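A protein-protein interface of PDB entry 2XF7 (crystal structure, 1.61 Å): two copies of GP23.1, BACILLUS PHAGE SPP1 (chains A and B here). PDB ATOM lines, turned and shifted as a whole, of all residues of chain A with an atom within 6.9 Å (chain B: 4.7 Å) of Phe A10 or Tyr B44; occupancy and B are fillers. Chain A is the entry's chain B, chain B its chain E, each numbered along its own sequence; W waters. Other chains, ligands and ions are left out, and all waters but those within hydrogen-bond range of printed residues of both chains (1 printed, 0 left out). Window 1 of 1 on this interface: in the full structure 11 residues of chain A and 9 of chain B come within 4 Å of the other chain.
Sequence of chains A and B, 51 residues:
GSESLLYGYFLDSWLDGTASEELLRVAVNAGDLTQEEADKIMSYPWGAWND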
ATOM      1  N   LEU A   6      11.686 -22.829 -15.424  1.00  0.00           N
ATOM      2  CA  LEU A   6      12.736 -22.926 -14.399  1.00  0.00           C
ATOM      3  C   LEU A   6      13.631 -21.728 -14.287  1.00  0.00           C
ATOM      4  O   LEU A   6      14.667 -21.779 -13.598  1.00  0.00           O
ATOM      5  CB  LEU A   6      13.568 -24.190 -14.679  1.00  0.00           C
ATOM      6  CG  LEU A   6      12.767 -25.507 -14.531  1.00  0.00           C
ATOM      7  CD1 LEU A   6      13.538 -26.686 -15.053  1.00  0.00           C
ATOM      8  CD2 LEU A   6      12.282 -25.715 -13.081  1.00  0.00           C
ATOM      9  N   TYR A   7      13.291 -20.635 -14.977  1.00  0.00           N
ATOM     10  CA  TYR A   7      14.126 -19.440 -14.853  1.00  0.00           C
ATOM     11  C   TYR A   7      14.349 -19.028 -13.340  1.00  0.00           C
ATOM     12  O   TYR A   7      15.505 -18.873 -12.885  1.00  0.00           O
ATOM     13  CB  TYR A   7      13.532 -18.282 -15.641  1.00  0.00           C
ATOM     14  CG  TYR A   7      14.385 -17.034 -15.548  1.00  0.00           C
ATOM     15  CD1 TYR A   7      15.544 -16.907 -16.289  1.00  0.00           C
ATOM     16  CD2 TYR A   7      14.122 -16.057 -14.589  1.00  0.00           C
ATOM     17  CE1 TYR A   7      16.350 -15.788 -16.167  1.00  0.00           C
ATOM     18  CE2 TYR A   7      14.919 -14.923 -14.454  1.00  0.00           C
ATOM     19  CZ  TYR A   7      16.028 -14.780 -15.262  1.00  0.00           C
ATOM     20  OH  TYR A   7      16.841 -13.691 -15.145  1.00  0.00           O
ATOM     21  N   GLY A   8      13.263 -18.894 -12.600  1.00  0.00           N
ATOM     22  CA  GLY A   8      13.382 -18.464 -11.204  1.00  0.00           C
ATOM     23  C   GLY A   8      14.160 -19.490 -10.400  1.00  0.00           C
ATOM     24  O   GLY A   8      14.938 -19.119  -9.488  1.00  0.00           O
ATOM     25  N   TYR A   9      13.896 -20.772 -10.666  1.00  0.00           N
ATOM     26  CA  TYR A   9      14.585 -21.845  -9.954  1.00  0.00           C
ATOM     27  C   TYR A   9      16.126 -21.677 -10.114  1.00  0.00           C
ATOM     28  O   TYR A   9      16.870 -21.753  -9.132  1.00  0.00           O
ATOM     29  CB  TYR A   9      14.152 -23.192 -10.544  1.00  0.00           C
ATOM     30  CG  TYR A   9      14.839 -24.346  -9.902  1.00  0.00           C
ATOM     31  CD1 TYR A   9      14.394 -24.848  -8.682  1.00  0.00           C
ATOM     32  CD2 TYR A   9      15.878 -25.008 -10.551  1.00  0.00           C
ATOM     33  CE1 TYR A   9      14.988 -25.963  -8.104  1.00  0.00           C
ATOM     34  CE2 TYR A   9      16.493 -26.119  -9.977  1.00  0.00           C
ATOM     35  CZ  TYR A   9      16.044 -26.585  -8.743  1.00  0.00           C
ATOM     36  OH  TYR A   9      16.624 -27.661  -8.118  1.00  0.00           O
ATOM     37  N   PHE A  10      16.610 -21.494 -11.362  1.00  0.00           N
ATOM     38  CA  PHE A  10      18.053 -21.368 -11.605  1.00  0.00           C
ATOM     39  C   PHE A  10      18.601 -20.025 -11.081  1.00  0.00           C
ATOM     40  O   PHE A  10      19.726 -19.979 -10.537  1.00  0.00           O
ATOM     41  CB  PHE A  10      18.403 -21.576 -13.076  1.00  0.00           C
ATOM     42  CG  PHE A  10      18.281 -23.052 -13.426  1.00  0.00           C
ATOM     43  CD1 PHE A  10      19.159 -23.985 -12.883  1.00  0.00           C
ATOM     44  CD2 PHE A  10      17.321 -23.494 -14.330  1.00  0.00           C
ATOM     45  CE1 PHE A  10      19.044 -25.377 -13.211  1.00  0.00           C
ATOM     46  CE2 PHE A  10      17.243 -24.886 -14.695  1.00  0.00           C
ATOM     47  CZ  PHE A  10      18.084 -25.795 -14.099  1.00  0.00           C
ATOM     48  N   LEU A  11      17.826 -18.978 -11.198  1.00  0.00           N
ATOM     49  CA  LEU A  11      18.277 -17.678 -10.645  1.00  0.00           C
ATOM     50  C   LEU A  11      18.464 -17.807  -9.132  1.00  0.00           C
ATOM     51  O   LEU A  11      19.462 -17.351  -8.562  1.00  0.00           O
ATOM     52  CB  LEU A  11      17.207 -16.629 -10.958  1.00  0.00           C
ATOM     53  CG  LEU A  11      17.446 -15.256 -10.287  1.00  0.00           C
ATOM     54  CD1 LEU A  11      18.826 -14.652 -10.704  1.00  0.00           C
ATOM     55  CD2 LEU A  11      16.283 -14.284 -10.670  1.00  0.00           C
ATOM     56  N   ASP A  12      17.501 -18.472  -8.452  1.00  0.00           N
ATOM     57  CA  ASP A  12      17.609 -18.646  -6.998  1.00  0.00           C
ATOM     58  C   ASP A  12      18.872 -19.446  -6.665  1.00  0.00           C
ATOM     59  O   ASP A  12      19.586 -19.107  -5.693  1.00  0.00           O
ATOM     60  CB  ASP A  12      16.327 -19.370  -6.511  1.00  0.00           C
ATOM     61  CG  ASP A  12      16.365 -19.565  -5.039  1.00  0.00           C
ATOM     62  OD1 ASP A  12      16.253 -18.567  -4.325  1.00  0.00           O
ATOM     63  OD2 ASP A  12      16.505 -20.749  -4.598  1.00  0.00           O
ATOM     64  N   SER A  13      19.193 -20.464  -7.492  1.00  0.00           N
ATOM     65  CA  SER A  13      20.401 -21.250  -7.247  1.00  0.00           C
ATOM     66  C   SER A  13      21.673 -20.429  -7.447  1.00  0.00           C
ATOM     67  O   SER A  13      22.663 -20.612  -6.707  1.00  0.00           O
ATOM     68  CB  SER A  13      20.409 -22.507  -8.111  1.00  0.00           C
ATOM     69  OG  SER A  13      19.332 -23.322  -7.683  1.00  0.00           O
ATOM     70  N   TRP A  14      21.656 -19.511  -8.391  1.00  0.00           N
ATOM     71  CA  TRP A  14      22.807 -18.633  -8.648  1.00  0.00           C
ATOM     72  C   TRP A  14      22.957 -17.676  -7.410  1.00  0.00           C
ATOM     73  O   TRP A  14      24.059 -17.582  -6.841  1.00  0.00           O
ATOM     74  CB  TRP A  14      22.533 -17.843  -9.897  1.00  0.00           C
ATOM     75  CG  TRP A  14      23.648 -16.887 -10.233  1.00  0.00           C
ATOM     76  CD1 TRP A  14      23.680 -15.536  -9.964  1.00  0.00           C
ATOM     77  CD2 TRP A  14      24.840 -17.179 -11.007  1.00  0.00           C
ATOM     78  NE1 TRP A  14      24.846 -14.987 -10.460  1.00  0.00           N
ATOM     79  CE2 TRP A  14      25.585 -15.973 -11.091  1.00  0.00           C
ATOM     80  CE3 TRP A  14      25.364 -18.342 -11.591  1.00  0.00           C
ATOM     81  CZ2 TRP A  14      26.806 -15.882 -11.817  1.00  0.00           C
ATOM     82  CZ3 TRP A  14      26.585 -18.271 -12.311  1.00  0.00           C
ATOM     83  CH2 TRP A  14      27.294 -17.055 -12.412  1.00  0.00           C
ATOM     84  N   LEU A  15      21.844 -17.031  -6.987  1.00  0.00           N
ATOM     85  CA  LEU A  15      21.864 -16.105  -5.824  1.00  0.00           C
ATOM     86  C   LEU A  15      22.285 -16.868  -4.554  1.00  0.00           C
ATOM     87  O   LEU A  15      22.915 -16.269  -3.712  1.00  0.00           O
ATOM     88  CB  LEU A  15      20.493 -15.456  -5.637  1.00  0.00           C
ATOM     89  CG  LEU A  15      20.168 -14.464  -6.787  1.00  0.00           C
ATOM     90  CD1 LEU A  15      18.709 -13.977  -6.757  1.00  0.00           C
ATOM     91  CD2 LEU A  15      21.119 -13.181  -6.690  1.00  0.00           C
ATOM     92  N   ASP A  16      21.898 -18.153  -4.388  1.00  0.00           N
ATOM     93  CA  ASP A  16      22.311 -18.864  -3.182  1.00  0.00           C
ATOM     94  C   ASP A  16      23.729 -19.481  -3.269  1.00  0.00           C
ATOM     95  O   ASP A  16      24.203 -20.088  -2.300  1.00  0.00           O
ATOM     96  CB  ASP A  16      21.204 -19.779  -2.630  1.00  0.00           C
ATOM     97  CG  ASP A  16      20.903 -20.993  -3.378  1.00  0.00           C
ATOM     98  OD1 ASP A  16      21.722 -21.358  -4.238  1.00  0.00           O
ATOM     99  OD2 ASP A  16      19.873 -21.659  -3.044  1.00  0.00           O
ATOM    100  N   THR A  18      24.741 -21.965  -5.116  1.00  0.00           N
ATOM    101  CA  THR A  18      24.819 -23.410  -5.331  1.00  0.00           C
ATOM    102  C   THR A  18      24.991 -23.730  -6.794  1.00  0.00           C
ATOM    103  O   THR A  18      25.328 -24.886  -7.143  1.00  0.00           O
ATOM    104  CB  THR A  18      23.540 -24.093  -4.754  1.00  0.00           C
ATOM    105  OG1 THR A  18      22.381 -23.501  -5.347  1.00  0.00           O
ATOM    106  CG2 THR A  18      23.445 -23.911  -3.218  1.00  0.00           C
ATOM    107  N   ALA A  19      24.754 -22.765  -7.666  1.00  0.00           N
ATOM    108  CA  ALA A  19      24.989 -22.959  -9.122  1.00  0.00           C
ATOM    109  C   ALA A  19      26.049 -21.995  -9.617  1.00  0.00           C
ATOM    110  O   ALA A  19      26.045 -20.818  -9.196  1.00  0.00           O
ATOM    111  CB  ALA A  19      23.723 -22.629  -9.930  1.00  0.00           C
ATOM    112  N   LEU A  23      26.497 -25.304 -14.216  1.00  0.00           N
ATOM    113  CA  LEU A  23      25.144 -25.776 -14.185  1.00  0.00           C
ATOM    114  C   LEU A  23      24.243 -25.043 -15.194  1.00  0.00           C
ATOM    115  O   LEU A  23      23.420 -25.598 -15.822  1.00  0.00           O
ATOM    116  CB  LEU A  23      24.653 -25.647 -12.761  1.00  0.00           C
ATOM    117  CG  LEU A  23      23.315 -26.178 -12.343  1.00  0.00           C
ATOM    118  CD1 LEU A  23      22.405 -25.375 -12.918  1.00  0.00           C
ATOM    119  CD2 LEU A  23      23.110 -27.542 -12.806  1.00  0.00           C
ATOM    120  N   LEU A  24      24.441 -23.724 -15.318  1.00  0.00           N
ATOM    121  CA  LEU A  24      23.652 -22.971 -16.301  1.00  0.00           C
ATOM    122  C   LEU A  24      23.936 -23.524 -17.722  1.00  0.00           C
ATOM    123  O   LEU A  24      23.002 -23.664 -18.513  1.00  0.00           O
ATOM    124  CB  LEU A  24      23.905 -21.436 -16.257  1.00  0.00           C
ATOM    125  CG  LEU A  24      23.636 -20.820 -14.869  1.00  0.00           C
ATOM    126  CD1 LEU A  24      23.886 -19.330 -14.935  1.00  0.00           C
ATOM    127  CD2 LEU A  24      22.182 -21.188 -14.340  1.00  0.00           C
ATOM    128  N   VAL A  26      24.699 -26.604 -18.549  1.00  0.00           N
ATOM    129  CA  VAL A  26      23.992 -27.875 -18.697  1.00  0.00           C
ATOM    130  C   VAL A  26      22.490 -27.552 -18.979  1.00  0.00           C
ATOM    131  O   VAL A  26      21.887 -28.161 -19.859  1.00  0.00           O
ATOM    132  CB  VAL A  26      24.163 -28.717 -17.396  1.00  0.00           C
ATOM    133  CG1 VAL A  26      23.188 -29.916 -17.383  1.00  0.00           C
ATOM    134  CG2 VAL A  26      25.617 -29.203 -17.216  1.00  0.00           C
ATOM    135  N   ALA A  27      21.915 -26.606 -18.243  1.00  0.00           N
ATOM    136  CA  ALA A  27      20.496 -26.243 -18.391  1.00  0.00           C
ATOM    137  C   ALA A  27      20.223 -25.677 -19.802  1.00  0.00           C
ATOM    138  O   ALA A  27      19.227 -26.040 -20.435  1.00  0.00           O
ATOM    139  CB  ALA A  27      20.085 -25.228 -17.332  1.00  0.00           C
ATOM    140  N   VAL A  28      21.130 -24.828 -20.323  1.00  0.00           N
ATOM    141  CA  VAL A  28      20.943 -24.290 -21.683  1.00  0.00           C
ATOM    142  C   VAL A  28      21.021 -25.432 -22.693  1.00  0.00           C
ATOM    143  O   VAL A  28      20.191 -25.509 -23.602  1.00  0.00           O
ATOM    144  CB  VAL A  28      22.010 -23.192 -21.989  1.00  0.00           C
ATOM    145  CG1 VAL A  28      21.962 -22.780 -23.462  1.00  0.00           C
ATOM    146  CG2 VAL A  28      21.742 -21.964 -21.122  1.00  0.00           C
ATOM    147  N   ALA A  30      20.386 -28.562 -22.297  1.00  0.00           N
ATOM    148  CA  ALA A  30      19.170 -29.380 -22.101  1.00  0.00           C
ATOM    149  C   ALA A  30      17.882 -28.724 -22.595  1.00  0.00           C
ATOM    150  O   ALA A  30      16.915 -29.421 -22.836  1.00  0.00           O
ATOM    151  CB  ALA A  30      19.007 -29.760 -20.622  1.00  0.00           C
ATOM    152  N   GLY A  31      17.925 -27.438 -22.861  1.00  0.00           N
ATOM    153  CA  GLY A  31      16.733 -26.689 -23.269  1.00  0.00           C
ATOM    154  C   GLY A  31      15.894 -26.268 -22.068  1.00  0.00           C
ATOM    155  O   GLY A  31      14.741 -25.856 -22.224  1.00  0.00           O
ATOM    156  N   ASP A  32      16.474 -26.307 -20.851  1.00  0.00           N
ATOM    157  CA  ASP A  32      15.711 -25.838 -19.679  1.00  0.00           C
ATOM    158  C   ASP A  32      15.821 -24.304 -19.420  1.00  0.00           C
ATOM    159  O   ASP A  32      15.074 -23.720 -18.587  1.00  0.00           O
ATOM    160  CB  ASP A  32      16.065 -26.621 -18.410  1.00  0.00           C
ATOM    161  CG  ASP A  32      15.571 -28.076 -18.461  1.00  0.00           C
ATOM    162  OD1 ASP A  32      14.549 -28.351 -19.142  1.00  0.00           O
ATOM    163  OD2 ASP A  32      16.245 -28.947 -17.883  1.00  0.00           O
ATOM    164  N   LEU A  33      16.818 -23.683 -20.093  1.00  0.00           N
ATOM    165  CA  LEU A  33      17.028 -22.228 -20.070  1.00  0.00           C
ATOM    166  C   LEU A  33      17.484 -21.877 -21.466  1.00  0.00           C
ATOM    167  O   LEU A  33      18.101 -22.711 -22.165  1.00  0.00           O
ATOM    168  CB  LEU A  33      18.192 -21.778 -19.146  1.00  0.00           C
ATOM    169  CG  LEU A  33      17.994 -21.849 -17.635  1.00  0.00           C
ATOM    170  CD1 LEU A  33      19.309 -21.408 -16.940  1.00  0.00           C
ATOM    171  CD2 LEU A  33      16.847 -20.924 -17.209  1.00  0.00           C
ATOM    172  N   ILE A  41      20.777 -14.335 -15.773  1.00  0.00           N
ATOM    173  CA  ILE A  41      21.084 -14.816 -14.423  1.00  0.00           C
ATOM    174  C   ILE A  41      22.527 -14.456 -14.013  1.00  0.00           C
ATOM    175  O   ILE A  41      22.717 -13.995 -12.888  1.00  0.00           O
ATOM    176  CB  ILE A  41      20.874 -16.340 -14.385  1.00  0.00           C
ATOM    177  CG1 ILE A  41      19.357 -16.615 -14.464  1.00  0.00           C
ATOM    178  CG2 ILE A  41      21.507 -16.922 -13.101  1.00  0.00           C
ATOM    179  CD1 ILE A  41      19.001 -18.118 -14.740  1.00  0.00           C
ATOM    180  N   TYR B   7       8.215 -32.066 -13.835  1.00  0.00           N
ATOM    181  CA  TYR B   7       9.611 -32.016 -14.326  1.00  0.00           C
ATOM    182  C   TYR B   7      10.541 -31.298 -13.310  1.00  0.00           C
ATOM    183  O   TYR B   7      11.543 -31.864 -12.916  1.00  0.00           O
ATOM    184  CB  TYR B   7       9.677 -31.315 -15.675  1.00  0.00           C
ATOM    185  CG  TYR B   7      11.114 -31.274 -16.195  1.00  0.00           C
ATOM    186  CD1 TYR B   7      11.721 -32.423 -16.714  1.00  0.00           C
ATOM    187  CD2 TYR B   7      11.881 -30.102 -16.114  1.00  0.00           C
ATOM    188  CE1 TYR B   7      13.054 -32.427 -17.113  1.00  0.00           C
ATOM    189  CE2 TYR B   7      13.223 -30.093 -16.528  1.00  0.00           C
ATOM    190  CZ  TYR B   7      13.782 -31.256 -17.081  1.00  0.00           C
ATOM    191  OH  TYR B   7      15.084 -31.282 -17.480  1.00  0.00           O
ATOM    192  N   LEU B  11      13.695 -32.847 -11.288  1.00  0.00           N
ATOM    193  CA  LEU B  11      15.033 -32.270 -11.539  1.00  0.00           C
ATOM    194  C   LEU B  11      15.614 -31.798 -10.238  1.00  0.00           C
ATOM    195  O   LEU B  11      16.769 -32.054  -9.962  1.00  0.00           O
ATOM    196  CB  LEU B  11      14.931 -31.117 -12.523  1.00  0.00           C
ATOM    197  CG  LEU B  11      16.227 -30.347 -12.768  1.00  0.00           C
ATOM    198  CD1 LEU B  11      17.378 -31.265 -13.306  1.00  0.00           C
ATOM    199  CD2 LEU B  11      15.967 -29.218 -13.748  1.00  0.00           C
ATOM    200  N   TRP B  14      16.890 -34.615  -8.219  1.00  0.00           N
ATOM    201  CA  TRP B  14      18.133 -35.150  -8.727  1.00  0.00           C
ATOM    202  C   TRP B  14      19.282 -34.220  -8.294  1.00  0.00           C
ATOM    203  O   TRP B  14      20.290 -34.686  -7.766  1.00  0.00           O
ATOM    204  CB  TRP B  14      18.060 -35.241 -10.244  1.00  0.00           C
ATOM    205  CG  TRP B  14      19.314 -35.729 -10.898  1.00  0.00           C
ATOM    206  CD1 TRP B  14      20.303 -34.971 -11.481  1.00  0.00           C
ATOM    207  CD2 TRP B  14      19.682 -37.105 -11.106  1.00  0.00           C
ATOM    208  NE1 TRP B  14      21.261 -35.803 -12.028  1.00  0.00           N
ATOM    209  CE2 TRP B  14      20.899 -37.111 -11.824  1.00  0.00           C
ATOM    210  CE3 TRP B  14      19.088 -38.330 -10.761  1.00  0.00           C
ATOM    211  CZ2 TRP B  14      21.546 -38.299 -12.199  1.00  0.00           C
ATOM    212  CZ3 TRP B  14      19.724 -39.513 -11.141  1.00  0.00           C
ATOM    213  CH2 TRP B  14      20.964 -39.488 -11.815  1.00  0.00           C
ATOM    214  N   LEU B  15      19.109 -32.896  -8.462  1.00  0.00           N
ATOM    215  CA  LEU B  15      20.100 -31.931  -8.072  1.00  0.00           C
ATOM    216  C   LEU B  15      20.391 -31.954  -6.584  1.00  0.00           C
ATOM    217  O   LEU B  15      21.521 -31.673  -6.209  1.00  0.00           O
ATOM    218  CB  LEU B  15      19.706 -30.525  -8.534  1.00  0.00           C
ATOM    219  CG  LEU B  15      19.731 -30.355 -10.063  1.00  0.00           C
ATOM    220  CD1 LEU B  15      19.100 -29.042 -10.468  1.00  0.00           C
ATOM    221  CD2 LEU B  15      21.215 -30.381 -10.617  1.00  0.00           C
ATOM    222  N   LYS B  40      17.164 -36.108 -19.851  1.00  0.00           N
ATOM    223  CA  LYS B  40      17.656 -34.712 -19.654  1.00  0.00           C
ATOM    224  C   LYS B  40      18.036 -34.527 -18.165  1.00  0.00           C
ATOM    225  O   LYS B  40      19.098 -33.996 -17.892  1.00  0.00           O
ATOM    226  CB  LYS B  40      16.610 -33.595 -19.913  1.00  0.00           C
ATOM    227  CG  LYS B  40      16.201 -33.342 -21.348  1.00  0.00           C
ATOM    228  CD  LYS B  40      15.457 -31.976 -21.439  1.00  0.00           C
ATOM    229  CE  LYS B  40      14.184 -31.778 -20.600  1.00  0.00           C
ATOM    230  NZ  LYS B  40      13.578 -30.381 -20.751  1.00  0.00           N
ATOM    231  N   ILE B  41      17.200 -34.965 -17.229  1.00  0.00           N
ATOM    232  CA  ILE B  41      17.563 -34.801 -15.822  1.00  0.00           C
ATOM    233  C   ILE B  41      18.870 -35.520 -15.501  1.00  0.00           C
ATOM    234  O   ILE B  41      19.715 -34.953 -14.811  1.00  0.00           O
ATOM    235  CB  ILE B  41      16.410 -35.318 -14.927  1.00  0.00           C
ATOM    236  CG1 ILE B  41      15.188 -34.368 -15.081  1.00  0.00           C
ATOM    237  CG2 ILE B  41      16.911 -35.438 -13.462  1.00  0.00           C
ATOM    238  CD1 ILE B  41      13.877 -34.904 -14.469  1.00  0.00           C
ATOM    239  N   MET B  42      19.059 -36.762 -16.015  1.00  0.00           N
ATOM    240  CA  MET B  42      20.275 -37.530 -15.705  1.00  0.00           C
ATOM    241  C   MET B  42      21.542 -36.909 -16.337  1.00  0.00           C
ATOM    242  O   MET B  42      22.649 -37.316 -15.979  1.00  0.00           O
ATOM    243  CB  MET B  42      20.101 -39.000 -16.063  1.00  0.00           C
ATOM    244  CG  MET B  42      19.038 -39.628 -15.195  1.00  0.00           C
ATOM    245  SD  MET B  42      18.958 -41.428 -15.418  1.00  0.00           S
ATOM    246  CE  MET B  42      18.074 -41.523 -16.901  1.00  0.00           C
ATOM    247  N   SER B  43      21.367 -35.907 -17.218  1.00  0.00           N
ATOM    248  CA  SER B  43      22.484 -35.180 -17.859  1.00  0.00           C
ATOM    249  C   SER B  43      23.076 -34.153 -16.883  1.00  0.00           C
ATOM    250  O   SER B  43      24.172 -33.595 -17.130  1.00  0.00           O
ATOM    251  CB  SER B  43      22.056 -34.535 -19.174  1.00  0.00           C
ATOM    252  OG  SER B  43      21.370 -33.298 -18.981  1.00  0.00           O
ATOM    253  N   TYR B  44      22.317 -33.806 -15.865  1.00  0.00           N
ATOM    254  CA  TYR B  44      22.753 -32.835 -14.838  1.00  0.00           C
ATOM    255  C   TYR B  44      23.574 -33.587 -13.789  1.00  0.00           C
ATOM    256  O   TYR B  44      23.404 -34.828 -13.610  1.00  0.00           O
ATOM    257  CB  TYR B  44      21.519 -32.254 -14.102  1.00  0.00           C
ATOM    258  CG  TYR B  44      20.772 -31.194 -14.873  1.00  0.00           C
ATOM    259  CD1 TYR B  44      20.942 -29.840 -14.578  1.00  0.00           C
ATOM    260  CD2 TYR B  44      19.821 -31.542 -15.829  1.00  0.00           C
ATOM    261  CE1 TYR B  44      20.193 -28.858 -15.226  1.00  0.00           C
ATOM    262  CE2 TYR B  44      19.065 -30.561 -16.495  1.00  0.00           C
ATOM    263  CZ  TYR B  44      19.246 -29.215 -16.167  1.00  0.00           C
ATOM    264  OH  TYR B  44      18.474 -28.197 -16.730  1.00  0.00           O
ATOM    265  N   PRO B  45      24.392 -32.818 -13.022  1.00  0.00           N
ATOM    266  CA  PRO B  45      25.229 -33.450 -11.967  1.00  0.00           C
ATOM    267  C   PRO B  45      24.353 -33.852 -10.777  1.00  0.00           C
ATOM    268  O   PRO B  45      23.712 -33.017 -10.135  1.00  0.00           O
ATOM    269  CB  PRO B  45      26.251 -32.322 -11.621  1.00  0.00           C
ATOM    270  CG  PRO B  45      25.569 -31.064 -11.954  1.00  0.00           C
ATOM    271  CD  PRO B  45      24.665 -31.365 -13.139  1.00  0.00           C
ATOM    272  N   TRP B  46      24.348 -35.140 -10.470  1.00  0.00           N
ATOM    273  CA  TRP B  46      23.586 -35.655  -9.337  1.00  0.00           C
ATOM    274  C   TRP B  46      24.135 -35.084  -8.043  1.00  0.00           C
ATOM    275  O   TRP B  46      25.351 -35.129  -7.775  1.00  0.00           O
ATOM    276  CB  TRP B  46      23.671 -37.183  -9.297  1.00  0.00           C
ATOM    277  CG  TRP B  46      22.893 -37.785  -8.185  1.00  0.00           C
ATOM    278  CD1 TRP B  46      21.548 -38.020  -8.152  1.00  0.00           C
ATOM    279  CD2 TRP B  46      23.431 -38.369  -6.998  1.00  0.00           C
ATOM    280  NE1 TRP B  46      21.204 -38.609  -6.970  1.00  0.00           N
ATOM    281  CE2 TRP B  46      22.342 -38.862  -6.246  1.00  0.00           C
ATOM    282  CE3 TRP B  46      24.729 -38.487  -6.469  1.00  0.00           C
ATOM    283  CZ2 TRP B  46      22.517 -39.551  -5.034  1.00  0.00           C
ATOM    284  CZ3 TRP B  46      24.905 -39.127  -5.250  1.00  0.00           C
ATOM    285  CH2 TRP B  46      23.812 -39.662  -4.544  1.00  0.00           C
HETATM  286  O   HOH W   1      22.141 -30.825 -20.495  1.00  0.00           O
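The side-chain carboxylate (OD2) of Asp A32 is in hydrogen-bond range of the side-chain hydroxyl (OH) of Tyr B44 (2.6 Å).
OH of Tyr B7 is in hydrogen-bond range of OD2 of Asp A32, at 2.6 Å.
NZ of Lys B40 is in salt-bridge range of OD1 of Asp A32.
The backbone carbonyl oxygen (O) of Ala A27 is in hydrogen-bond range of the backbone NH (N) of Leu A33 (3.4 Å).
The side-chain hydroxyl (OG) of Ser B43 sits at hydrogen-bond distance from the backbone carbonyl oxygen (O) of Lys B40 (2.6 Å).
The side-chain hydroxyl (OG) of Ser A13 is in hydrogen-bond range of the backbone carbonyl oxygen (O) of Tyr A9, 3.3 Å away.
The indole nitrogen (NE1) of Trp B14 lies within hydrogen-bond range of the backbone carbonyl oxygen (O) of Tyr B44 (2.8 Å).
The backbone carbonyl oxygen (O) of Ala A27 lies within hydrogen-bond range of the backbone NH (N) of Asp A32, at 2.8 Å.
Tyr B7 touches Leu A6.
CD1 of Leu A6 touches CD2 of Leu B11 (3.7 Å).
CD1 of Leu B15 touches OH of Tyr A9, 3.7 Å away.
Tyr B44 touches Phe A10.
CD2 of Leu A23 touches CD1 of Tyr B44, at 3.6 Å.
O of Ser B43 touches CG1 of Val A26 (3.8 Å).
Val A26 touches Tyr B44.
Ala A27 touches Tyr B44.
Ala A30 touches Lys B40 (O to CD, 3.3 Å).
Of the printed residues of chain B, Tyr A9 touches Leu B15.
Phe A10 touches just one residue of chain B: Tyr B44.
Leu A11 touches none of the printed residues of chain B.
Printed residues of chain B within 4 Å of Val A26: Ser B43 (3.8 Å) and Tyr B44 (3.6 Å).
Of the printed residues of chain B, Ala A27 touches Tyr B44.
Of the printed residues of chain A, Tyr B7 touches Leu A6 and Asp A32.
Met B42 touches none of the printed residues of chain A.
Printed residues of chain A within 4 Å of Tyr B44: Phe A10 (3.6 Å), Leu A23 (3.6 Å), Val A26 (3.6 Å), Ala A27 (3.3 Å) and Asp A32 (2.6 Å).
The nearest printed residue of chain A that does not touch Tyr B44 is Ala A30 (4.2 Å).
Hydrophobic or aromatic side chains of chain B within 4 Å of the printed part of chain A: Tyr B7, Leu B11, Leu B15 and Tyr B44.
Printed residues of chain A that touch a printed residue of chain B: Leu A6, Tyr A9, Phe A10, Leu A23, Val A26, Ala A27, Ala A30 and Asp A32.
5 positions are printed for both chains.
Of the 12 pairs that touch across the chains among the printed residues, none has its exchanged pair printed and touching as well.
Water W1 lies within hydrogen-bond range of the backbone carbonyl oxygen of Val A26 (2.8 Å), the side-chain hydroxyl of Ser B43 (3.0 Å) and the backbone NH of Ala A30 (3.4 Å).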
